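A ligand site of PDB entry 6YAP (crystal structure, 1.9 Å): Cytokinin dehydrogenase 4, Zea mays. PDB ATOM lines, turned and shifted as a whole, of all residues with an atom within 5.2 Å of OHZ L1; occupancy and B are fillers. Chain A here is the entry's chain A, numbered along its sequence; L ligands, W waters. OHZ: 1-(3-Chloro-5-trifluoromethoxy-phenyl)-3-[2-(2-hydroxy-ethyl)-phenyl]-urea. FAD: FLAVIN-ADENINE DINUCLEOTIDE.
O4 of FAD L2 is in hydrogen-bond range of N1 of OHZ L1, 3.2 Å away.
Ile 185 touches OHZ L1 (O to C14, 3.97 Å). Glu 285 touches OHZ L1 (OE2 to O2, 3.7 Å). Val 370 touches OHZ L1 (CG1 to C5, 3.6 Å). Leu 377 touches OHZ L1 (CD1 to F, 3.4 Å). CZ3 of Trp 383 touches F of OHZ L1, at 3.6 Å. CZ2 of Trp 389 touches F1 of OHZ L1, 3.0 Å away. OD1 of Asn 391 touches C11 of OHZ L1, at 3.3 Å. Leu 423 touches OHZ L1 (CD1 to O2, 3.4 Å). Leu 448 touches OHZ L1 (CD2 to C15, 3.6 Å). CD1 of Leu 452 touches C of OHZ L1, at 3.3 Å. CE2 of Tyr 487 touches C12 of OHZ L1, 3.8 Å away. Leu 488 touches OHZ L1. Hydrophobic or aromatic side chains that line OHZ L1: Val 370, Leu 377, Trp 383, Trp 389, Leu 423, Tyr 425, Leu 448, Leu 452, Tyr 487 and Leu 488. 14 residues have an atom within 4 Å of OHZ L1: Asp 170, Ile 185, Glu 285, Val 370, Leu 377, Trp 383, Trp 389, Asn 391, Leu 423, Tyr 425, Leu 448, Leu 452, Tyr 487 and Leu 488. The nearest printed residue that does not touch OHZ L1 is Ala 450 (4.03 Å).
The backbone NH of Leu 452 is in hydrogen-bond range of the backbone carbonyl oxygen of Pro 421, at 2.9 Å. OD1 of Asp 170 sits at hydrogen-bond distance from OG of Ser 186, at 2.9 Å. The backbone NH of Tyr 487 lies within hydrogen-bond range of the backbone carbonyl oxygen of Asn 391 (2.9 Å). OD1 of Asp 170 sits close to OE1 of Glu 285 (2.6 Å). O of Tyr 425 lies within hydrogen-bond range of N of Leu 448 (2.9 Å). OE1 of Glu 285 lies within hydrogen-bond range of OG of Ser 186. N of Ala 450 lies within hydrogen-bond range of O of Leu 423.
The side-chain hydroxyl (OH) of Tyr 487 lies within hydrogen-bond range of an oxygen (O2) of FAD L2 (2.6 Å). The backbone NH of Ile 185 lies within hydrogen-bond range of an oxygen (O2) of FAD L2. The backbone carbonyl oxygen (O) of Ile 185 is in hydrogen-bond range of a nitrogen (N3) of FAD L2. OH of Tyr 425 sits at hydrogen-bond distance from O2 of OHZ L1 (2.8 Å). O2 of OHZ L1 sits at hydrogen-bond distance from OD2 of Asp 170, at 2.7 Å. An oxygen (O4) of FAD L2 sits at hydrogen-bond distance from the backbone NH (N) of Asp 170, at 2.7 Å.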
ATOM      1  N   PHE A  57       5.171 -28.797  18.772  1.00  0.00           N
ATOM      2  CA  PHE A  57       6.254 -28.207  17.993  1.00  0.00           C
ATOM      3  C   PHE A  57       7.060 -27.160  18.808  1.00  0.00           C
ATOM      4  O   PHE A  57       8.252 -26.997  18.542  1.00  0.00           O
ATOM      5  CB  PHE A  57       5.667 -27.595  16.733  1.00  0.00           C
ATOM      6  CG  PHE A  57       6.664 -27.020  15.765  1.00  0.00           C
ATOM      7  CD1 PHE A  57       7.394 -27.842  14.919  1.00  0.00           C
ATOM      8  CD2 PHE A  57       6.817 -25.631  15.653  1.00  0.00           C
ATOM      9  CE1 PHE A  57       8.244 -27.305  13.955  1.00  0.00           C
ATOM     10  CE2 PHE A  57       7.642 -25.095  14.669  1.00  0.00           C
ATOM     11  CZ  PHE A  57       8.355 -25.932  13.820  1.00  0.00           C
ATOM     12  N   ASP A 170       1.151 -21.390   5.102  1.00  0.00           N
ATOM     13  CA  ASP A 170       2.431 -21.594   4.403  1.00  0.00           C
ATOM     14  C   ASP A 170       2.802 -23.072   4.461  1.00  0.00           C
ATOM     15  O   ASP A 170       3.490 -23.563   3.582  1.00  0.00           O
ATOM     16  CB  ASP A 170       3.571 -20.818   5.143  1.00  0.00           C
ATOM     17  CG  ASP A 170       3.515 -19.305   5.155  1.00  0.00           C
ATOM     18  OD1 ASP A 170       2.757 -18.723   4.339  1.00  0.00           O
ATOM     19  OD2 ASP A 170       4.232 -18.694   5.965  1.00  0.00           O
ATOM     20  N   ILE A 185      -3.567 -18.437   7.970  1.00  0.00           N
ATOM     21  CA  ILE A 185      -3.097 -17.293   7.203  1.00  0.00           C
ATOM     22  C   ILE A 185      -1.901 -17.619   6.305  1.00  0.00           C
ATOM     23  O   ILE A 185      -1.024 -18.374   6.709  1.00  0.00           O
ATOM     24  CB  ILE A 185      -2.722 -16.130   8.184  1.00  0.00           C
ATOM     25  CG1 ILE A 185      -3.875 -15.802   9.172  1.00  0.00           C
ATOM     26  CG2 ILE A 185      -2.293 -14.874   7.433  1.00  0.00           C
ATOM     27  CD1 ILE A 185      -3.407 -14.893  10.354  1.00  0.00           C
ATOM     28  N   SER A 186      -1.842 -16.975   5.139  1.00  0.00           N
ATOM     29  CA  SER A 186      -0.732 -17.072   4.186  1.00  0.00           C
ATOM     30  C   SER A 186      -0.857 -15.887   3.230  1.00  0.00           C
ATOM     31  O   SER A 186      -1.664 -15.004   3.491  1.00  0.00           O
ATOM     32  CB  SER A 186      -0.709 -18.413   3.454  1.00  0.00           C
ATOM     33  OG  SER A 186       0.435 -18.519   2.632  1.00  0.00           O
ATOM     34  N   ARG A 254      10.621 -13.235  -6.240  1.00  0.00           N
ATOM     35  CA  ARG A 254      11.264 -12.593  -5.091  1.00  0.00           C
ATOM     36  C   ARG A 254      12.077 -11.429  -5.588  1.00  0.00           C
ATOM     37  O   ARG A 254      12.732 -11.542  -6.627  1.00  0.00           O
ATOM     38  CB  ARG A 254      12.136 -13.559  -4.296  1.00  0.00           C
ATOM     39  CG  ARG A 254      11.329 -14.490  -3.419  1.00  0.00           C
ATOM     40  CD  ARG A 254      12.248 -15.475  -2.748  1.00  0.00           C
ATOM     41  NE  ARG A 254      11.498 -16.381  -1.875  1.00  0.00           N
ATOM     42  CZ  ARG A 254      12.046 -17.300  -1.094  1.00  0.00           C
ATOM     43  NH1 ARG A 254      11.289 -18.067  -0.327  1.00  0.00           N
ATOM     44  NH2 ARG A 254      13.370 -17.443  -1.057  1.00  0.00           N
ATOM     45  N   GLU A 285       3.636 -12.005   0.244  1.00  0.00           N
ATOM     46  CA  GLU A 285       4.344 -12.164   1.506  1.00  0.00           C
ATOM     47  C   GLU A 285       5.617 -11.321   1.464  1.00  0.00           C
ATOM     48  O   GLU A 285       5.808 -10.518   0.550  1.00  0.00           O
ATOM     49  CB  GLU A 285       4.619 -13.635   1.878  1.00  0.00           C
ATOM     50  CG  GLU A 285       3.353 -14.368   2.289  1.00  0.00           C
ATOM     51  CD  GLU A 285       3.564 -15.613   3.103  1.00  0.00           C
ATOM     52  OE1 GLU A 285       2.593 -16.378   3.254  1.00  0.00           O
ATOM     53  OE2 GLU A 285       4.704 -15.848   3.561  1.00  0.00           O
ATOM     54  N   VAL A 370       7.229 -25.447   2.124  1.00  0.00           N
ATOM     55  CA  VAL A 370       7.702 -25.494   3.518  1.00  0.00           C
ATOM     56  C   VAL A 370       7.974 -26.955   3.960  1.00  0.00           C
ATOM     57  O   VAL A 370       8.892 -27.197   4.762  1.00  0.00           O
ATOM     58  CB  VAL A 370       6.785 -24.687   4.498  1.00  0.00           C
ATOM     59  CG1 VAL A 370       7.248 -24.810   5.950  1.00  0.00           C
ATOM     60  CG2 VAL A 370       6.714 -23.222   4.082  1.00  0.00           C
ATOM     61  N   ALA A 373      11.486 -27.727   2.987  1.00  0.00           N
ATOM     62  CA  ALA A 373      12.386 -27.105   3.936  1.00  0.00           C
ATOM     63  C   ALA A 373      12.475 -28.007   5.193  1.00  0.00           C
ATOM     64  O   ALA A 373      13.573 -28.205   5.714  1.00  0.00           O
ATOM     65  CB  ALA A 373      11.904 -25.708   4.304  1.00  0.00           C
ATOM     66  N   LEU A 377      15.601 -30.041   7.157  1.00  0.00           N
ATOM     67  CA  LEU A 377      15.839 -29.758   8.573  1.00  0.00           C
ATOM     68  C   LEU A 377      15.922 -31.044   9.370  1.00  0.00           C
ATOM     69  O   LEU A 377      16.798 -31.179  10.233  1.00  0.00           O
ATOM     70  CB  LEU A 377      14.782 -28.807   9.171  1.00  0.00           C
ATOM     71  CG  LEU A 377      14.874 -27.331   8.750  1.00  0.00           C
ATOM     72  CD1 LEU A 377      13.549 -26.599   8.974  1.00  0.00           C
ATOM     73  CD2 LEU A 377      16.023 -26.609   9.466  1.00  0.00           C
ATOM     74  N   TRP A 383      14.969 -30.065  13.191  1.00  0.00           N
ATOM     75  CA  TRP A 383      13.510 -29.968  13.169  1.00  0.00           C
ATOM     76  C   TRP A 383      12.906 -30.176  14.539  1.00  0.00           C
ATOM     77  O   TRP A 383      12.069 -29.385  14.953  1.00  0.00           O
ATOM     78  CB  TRP A 383      12.895 -30.934  12.141  1.00  0.00           C
ATOM     79  CG  TRP A 383      11.397 -30.864  12.062  1.00  0.00           C
ATOM     80  CD1 TRP A 383      10.505 -31.727  12.621  1.00  0.00           C
ATOM     81  CD2 TRP A 383      10.622 -29.876  11.362  1.00  0.00           C
ATOM     82  NE1 TRP A 383       9.219 -31.351  12.318  1.00  0.00           N
ATOM     83  CE2 TRP A 383       9.258 -30.217  11.540  1.00  0.00           C
ATOM     84  CE3 TRP A 383      10.941 -28.718  10.636  1.00  0.00           C
ATOM     85  CZ2 TRP A 383       8.217 -29.436  11.017  1.00  0.00           C
ATOM     86  CZ3 TRP A 383       9.913 -27.962  10.098  1.00  0.00           C
ATOM     87  CH2 TRP A 383       8.564 -28.335  10.283  1.00  0.00           C
ATOM     88  N   TRP A 389       8.243 -19.523  18.874  1.00  0.00           N
ATOM     89  CA  TRP A 389       7.676 -18.701  17.806  1.00  0.00           C
ATOM     90  C   TRP A 389       6.780 -17.625  18.327  1.00  0.00           C
ATOM     91  O   TRP A 389       6.000 -17.874  19.237  1.00  0.00           O
ATOM     92  CB  TRP A 389       6.917 -19.577  16.785  1.00  0.00           C
ATOM     93  CG  TRP A 389       7.853 -20.348  15.899  1.00  0.00           C
ATOM     94  CD1 TRP A 389       9.212 -20.410  15.990  1.00  0.00           C
ATOM     95  CD2 TRP A 389       7.489 -21.111  14.736  1.00  0.00           C
ATOM     96  NE1 TRP A 389       9.721 -21.177  14.965  1.00  0.00           N
ATOM     97  CE2 TRP A 389       8.679 -21.595  14.167  1.00  0.00           C
ATOM     98  CE3 TRP A 389       6.269 -21.393  14.105  1.00  0.00           C
ATOM     99  CZ2 TRP A 389       8.692 -22.344  12.990  1.00  0.00           C
ATOM    100  CZ3 TRP A 389       6.275 -22.160  12.952  1.00  0.00           C
ATOM    101  CH2 TRP A 389       7.476 -22.610  12.397  1.00  0.00           C
ATOM    102  N   ASN A 391       4.052 -14.541  16.956  1.00  0.00           N
ATOM    103  CA  ASN A 391       3.290 -13.994  15.838  1.00  0.00           C
ATOM    104  C   ASN A 391       2.461 -12.823  16.282  1.00  0.00           C
ATOM    105  O   ASN A 391       1.641 -12.936  17.187  1.00  0.00           O
ATOM    106  CB  ASN A 391       2.400 -15.105  15.191  1.00  0.00           C
ATOM    107  CG  ASN A 391       3.236 -16.271  14.715  1.00  0.00           C
ATOM    108  OD1 ASN A 391       3.862 -16.202  13.694  1.00  0.00           O
ATOM    109  ND2 ASN A 391       3.317 -17.327  15.471  1.00  0.00           N
ATOM    110  N   PRO A 421      13.291 -17.805   9.930  1.00  0.00           N
ATOM    111  CA  PRO A 421      12.779 -16.619   9.235  1.00  0.00           C
ATOM    112  C   PRO A 421      11.964 -15.652  10.095  1.00  0.00           C
ATOM    113  O   PRO A 421      11.451 -15.995  11.171  1.00  0.00           O
ATOM    114  CB  PRO A 421      11.956 -17.210   8.080  1.00  0.00           C
ATOM    115  CG  PRO A 421      11.516 -18.536   8.564  1.00  0.00           C
ATOM    116  CD  PRO A 421      12.539 -19.017   9.557  1.00  0.00           C
ATOM    117  N   LEU A 423       8.949 -13.255   9.011  1.00  0.00           N
ATOM    118  CA  LEU A 423       8.042 -12.910   7.920  1.00  0.00           C
ATOM    119  C   LEU A 423       7.255 -11.663   8.242  1.00  0.00           C
ATOM    120  O   LEU A 423       6.997 -11.379   9.408  1.00  0.00           O
ATOM    121  CB  LEU A 423       7.079 -14.090   7.580  1.00  0.00           C
ATOM    122  CG  LEU A 423       7.675 -15.516   7.365  1.00  0.00           C
ATOM    123  CD1 LEU A 423       6.686 -16.414   6.674  1.00  0.00           C
ATOM    124  CD2 LEU A 423       8.923 -15.494   6.501  1.00  0.00           C
ATOM    125  N   TYR A 425       4.040  -9.112   6.211  1.00  0.00           N
ATOM    126  CA  TYR A 425       3.152  -8.748   5.114  1.00  0.00           C
ATOM    127  C   TYR A 425       1.823  -8.208   5.618  1.00  0.00           C
ATOM    128  O   TYR A 425       1.314  -8.645   6.655  1.00  0.00           O
ATOM    129  CB  TYR A 425       2.946  -9.906   4.088  1.00  0.00           C
ATOM    130  CG  TYR A 425       2.449 -11.211   4.670  1.00  0.00           C
ATOM    131  CD1 TYR A 425       3.342 -12.176   5.133  1.00  0.00           C
ATOM    132  CD2 TYR A 425       1.086 -11.492   4.739  1.00  0.00           C
ATOM    133  CE1 TYR A 425       2.888 -13.376   5.663  1.00  0.00           C
ATOM    134  CE2 TYR A 425       0.619 -12.719   5.235  1.00  0.00           C
ATOM    135  CZ  TYR A 425       1.521 -13.672   5.658  1.00  0.00           C
ATOM    136  OH  TYR A 425       1.072 -14.873   6.164  1.00  0.00           O
ATOM    137  N   LEU A 448       0.994  -9.045   9.550  1.00  0.00           N
ATOM    138  CA  LEU A 448       1.357 -10.188  10.356  1.00  0.00           C
ATOM    139  C   LEU A 448       2.878 -10.092  10.395  1.00  0.00           C
ATOM    140  O   LEU A 448       3.512  -9.883   9.361  1.00  0.00           O
ATOM    141  CB  LEU A 448       0.932 -11.520   9.733  1.00  0.00           C
ATOM    142  CG  LEU A 448       1.550 -12.812  10.336  1.00  0.00           C
ATOM    143  CD1 LEU A 448       1.177 -13.000  11.828  1.00  0.00           C
ATOM    144  CD2 LEU A 448       1.085 -14.010   9.543  1.00  0.00           C
ATOM    145  N   ALA A 450       5.829 -12.400  11.773  1.00  0.00           N
ATOM    146  CA  ALA A 450       6.053 -13.748  12.317  1.00  0.00           C
ATOM    147  C   ALA A 450       7.517 -13.998  12.612  1.00  0.00           C
ATOM    148  O   ALA A 450       8.338 -14.049  11.692  1.00  0.00           O
ATOM    149  CB  ALA A 450       5.485 -14.806  11.339  1.00  0.00           C
ATOM    150  N   LEU A 452       9.843 -16.554  13.538  1.00  0.00           N
ATOM    151  CA  LEU A 452       9.890 -18.028  13.449  1.00  0.00           C
ATOM    152  C   LEU A 452      11.289 -18.559  13.691  1.00  0.00           C
ATOM    153  O   LEU A 452      11.880 -19.227  12.848  1.00  0.00           O
ATOM    154  CB  LEU A 452       9.307 -18.489  12.068  1.00  0.00           C
ATOM    155  CG  LEU A 452       7.935 -17.914  11.677  1.00  0.00           C
ATOM    156  CD1 LEU A 452       7.485 -18.430  10.348  1.00  0.00           C
ATOM    157  CD2 LEU A 452       6.863 -18.213  12.741  1.00  0.00           C
ATOM    158  N   TYR A 487      -1.259 -13.378  17.406  1.00  0.00           N
ATOM    159  CA  TYR A 487      -1.922 -14.441  16.636  1.00  0.00           C
ATOM    160  C   TYR A 487      -1.381 -15.714  17.329  1.00  0.00           C
ATOM    161  O   TYR A 487      -0.212 -15.724  17.727  1.00  0.00           O
ATOM    162  CB  TYR A 487      -1.498 -14.409  15.150  1.00  0.00           C
ATOM    163  CG  TYR A 487      -2.043 -15.574  14.344  1.00  0.00           C
ATOM    164  CD1 TYR A 487      -3.406 -15.895  14.372  1.00  0.00           C
ATOM    165  CD2 TYR A 487      -1.221 -16.307  13.487  1.00  0.00           C
ATOM    166  CE1 TYR A 487      -3.919 -16.955  13.623  1.00  0.00           C
ATOM    167  CE2 TYR A 487      -1.725 -17.370  12.727  1.00  0.00           C
ATOM    168  CZ  TYR A 487      -3.073 -17.682  12.803  1.00  0.00           C
ATOM    169  OH  TYR A 487      -3.591 -18.700  12.045  1.00  0.00           O
ATOM    170  N   LEU A 488      -2.244 -16.735  17.547  1.00  0.00           N
ATOM    171  CA  LEU A 488      -1.941 -17.984  18.335  1.00  0.00           C
ATOM    172  C   LEU A 488      -1.532 -17.486  19.753  1.00  0.00           C
ATOM    173  O   LEU A 488      -0.413 -17.764  20.200  1.00  0.00           O
ATOM    174  CB  LEU A 488      -0.792 -18.811  17.676  1.00  0.00           C
ATOM    175  CG  LEU A 488      -0.854 -19.018  16.165  1.00  0.00           C
ATOM    176  CD1 LEU A 488       0.407 -19.679  15.630  1.00  0.00           C
ATOM    177  CD2 LEU A 488      -2.084 -19.807  15.766  1.00  0.00           C
HETATM  178  C1  OHZ L   1       7.289 -20.925   7.191  1.00  0.00           C
HETATM  179  C2  OHZ L   1       7.861 -20.340   6.076  1.00  0.00           C
HETATM  180  C3  OHZ L   1       9.094 -20.763   5.624  1.00  0.00           C
HETATM  181  C4  OHZ L   1       9.804 -21.710   6.321  1.00  0.00           C
HETATM  182  C5  OHZ L   1       9.298 -22.232   7.501  1.00  0.00           C
HETATM  183  C6  OHZ L   1       9.889 -23.729   9.348  1.00  0.00           C
HETATM  184  C7  OHZ L   1       8.034 -21.815   7.963  1.00  0.00           C
HETATM  185  C9  OHZ L   1       3.684 -19.860  11.338  1.00  0.00           C
HETATM  186  C10 OHZ L   1       2.868 -19.549  12.429  1.00  0.00           C
HETATM  187  C11 OHZ L   1       1.896 -18.529  12.308  1.00  0.00           C
HETATM  188  C12 OHZ L   1       1.695 -17.877  11.093  1.00  0.00           C
HETATM  189  C14 OHZ L   1       2.305 -17.469   8.682  1.00  0.00           C
HETATM  190  F2  OHZ L   1       8.733 -24.457   9.342  1.00  0.00           F
HETATM  191  F   OHZ L   1      10.918 -24.546   9.691  1.00  0.00           F
HETATM  192  F1  OHZ L   1       9.859 -22.683  10.224  1.00  0.00           F
HETATM  193  O1  OHZ L   1      10.132 -23.222   8.066  1.00  0.00           O
HETATM  194 CL   OHZ L   1       9.761 -20.129   4.094  1.00  0.00          CL
HETATM  195  N   OHZ L   1       6.062 -20.279   7.599  1.00  0.00           N
HETATM  196  C   OHZ L   1       5.358 -20.408   8.830  1.00  0.00           C
HETATM  197  O   OHZ L   1       5.660 -21.171   9.683  1.00  0.00           O
HETATM  198  N1  OHZ L   1       4.287 -19.469   8.950  1.00  0.00           N
HETATM  199  C8  OHZ L   1       3.442 -19.241  10.112  1.00  0.00           C
HETATM  200  C13 OHZ L   1       2.533 -18.175  10.018  1.00  0.00           C
HETATM  201  C15 OHZ L   1       3.413 -16.485   8.311  1.00  0.00           C
HETATM  202  O2  OHZ L   1       3.321 -16.314   6.918  1.00  0.00           O
HETATM  203  PA  FAD L   2      -2.965 -28.280  17.308  1.00  0.00           P
HETATM  204  O1A FAD L   2      -1.692 -27.549  17.528  1.00  0.00           O
HETATM  205  O2A FAD L   2      -2.891 -29.767  17.646  1.00  0.00           O
HETATM  206  O5B FAD L   2      -4.202 -27.657  18.087  1.00  0.00           O
HETATM  207  C5B FAD L   2      -4.282 -26.212  18.208  1.00  0.00           C
HETATM  208  C4B FAD L   2      -5.463 -25.830  19.074  1.00  0.00           C
HETATM  209  O4B FAD L   2      -6.688 -26.192  18.385  1.00  0.00           O
HETATM  210  C3B FAD L   2      -5.528 -26.530  20.426  1.00  0.00           C
HETATM  211  O3B FAD L   2      -6.135 -25.697  21.418  1.00  0.00           O
HETATM  212  C2B FAD L   2      -6.360 -27.769  20.110  1.00  0.00           C
HETATM  213  O2B FAD L   2      -6.938 -28.400  21.254  1.00  0.00           O
HETATM  214  C1B FAD L   2      -7.371 -27.190  19.114  1.00  0.00           C
HETATM  215  N9A FAD L   2      -7.936 -28.138  18.152  1.00  0.00           N
HETATM  216  C8A FAD L   2      -7.259 -29.034  17.364  1.00  0.00           C
HETATM  217  N7A FAD L   2      -8.018 -29.678  16.505  1.00  0.00           N
HETATM  218  C5A FAD L   2      -9.285 -29.192  16.763  1.00  0.00           C
HETATM  219  C6A FAD L   2     -10.556 -29.525  16.244  1.00  0.00           C
HETATM  220  N6A FAD L   2     -10.745 -30.442  15.292  1.00  0.00           N
HETATM  221  N1A FAD L   2     -11.630 -28.874  16.740  1.00  0.00           N
HETATM  222  C2A FAD L   2     -11.446 -27.945  17.687  1.00  0.00           C
HETATM  223  N3A FAD L   2     -10.299 -27.543  18.242  1.00  0.00           N
HETATM  224  C4A FAD L   2      -9.255 -28.224  17.754  1.00  0.00           C
HETATM  225  N1  FAD L   2      -0.479 -20.994  10.990  1.00  0.00           N
HETATM  226  C2  FAD L   2      -0.924 -20.161  10.029  1.00  0.00           C
HETATM  227  O2  FAD L   2      -2.000 -19.556  10.153  1.00  0.00           O
HETATM  228  N3  FAD L   2      -0.195 -20.015   8.880  1.00  0.00           N
HETATM  229  C4  FAD L   2       0.967 -20.680   8.578  1.00  0.00           C
HETATM  230  O4  FAD L   2       1.549 -20.433   7.543  1.00  0.00           O
HETATM  231  C4X FAD L   2       1.415 -21.603   9.590  1.00  0.00           C
HETATM  232  N5  FAD L   2       2.515 -22.287   9.368  1.00  0.00           N
HETATM  233  C5X FAD L   2       2.934 -23.156  10.358  1.00  0.00           C
HETATM  234  C6  FAD L   2       4.100 -23.912  10.144  1.00  0.00           C
HETATM  235  C7  FAD L   2       4.562 -24.812  11.100  1.00  0.00           C
HETATM  236  C7M FAD L   2       5.854 -25.549  10.849  1.00  0.00           C
HETATM  237  C8  FAD L   2       3.842 -24.973  12.304  1.00  0.00           C
HETATM  238  C8M FAD L   2       4.289 -25.942  13.358  1.00  0.00           C
HETATM  239  C9  FAD L   2       2.707 -24.205  12.523  1.00  0.00           C
HETATM  240  C9A FAD L   2       2.245 -23.293  11.576  1.00  0.00           C
HETATM  241  N10 FAD L   2       1.090 -22.493  11.774  1.00  0.00           N
HETATM  242  C10 FAD L   2       0.640 -21.671  10.792  1.00  0.00           C
HETATM  243  C1' FAD L   2       0.385 -22.482  13.078  1.00  0.00           C
HETATM  244  C2' FAD L   2      -0.853 -23.377  13.119  1.00  0.00           C
HETATM  245  O2' FAD L   2      -1.951 -22.771  12.443  1.00  0.00           O
HETATM  246  C3' FAD L   2      -1.257 -23.699  14.558  1.00  0.00           C
HETATM  247  O3' FAD L   2      -0.200 -24.421  15.178  1.00  0.00           O
HETATM  248  C4' FAD L   2      -2.590 -24.417  14.783  1.00  0.00           C
HETATM  249  O4' FAD L   2      -2.705 -24.784  16.151  1.00  0.00           O
HETATM  250  C5' FAD L   2      -2.829 -25.612  13.871  1.00  0.00           C
HETATM  251  O5' FAD L   2      -1.898 -26.675  14.176  1.00  0.00           O
HETATM  252  P   FAD L   2      -2.510 -28.152  14.439  1.00  0.00           P
HETATM  253  O1P FAD L   2      -3.333 -28.686  13.348  1.00  0.00           O
HETATM  254  O2P FAD L   2      -1.340 -29.076  14.737  1.00  0.00           O
HETATM  255  O3P FAD L   2      -3.371 -28.084  15.774  1.00  0.00           O
HETATM  256  O   HOH W   1      10.589 -21.607   1.218  1.00  0.00           O
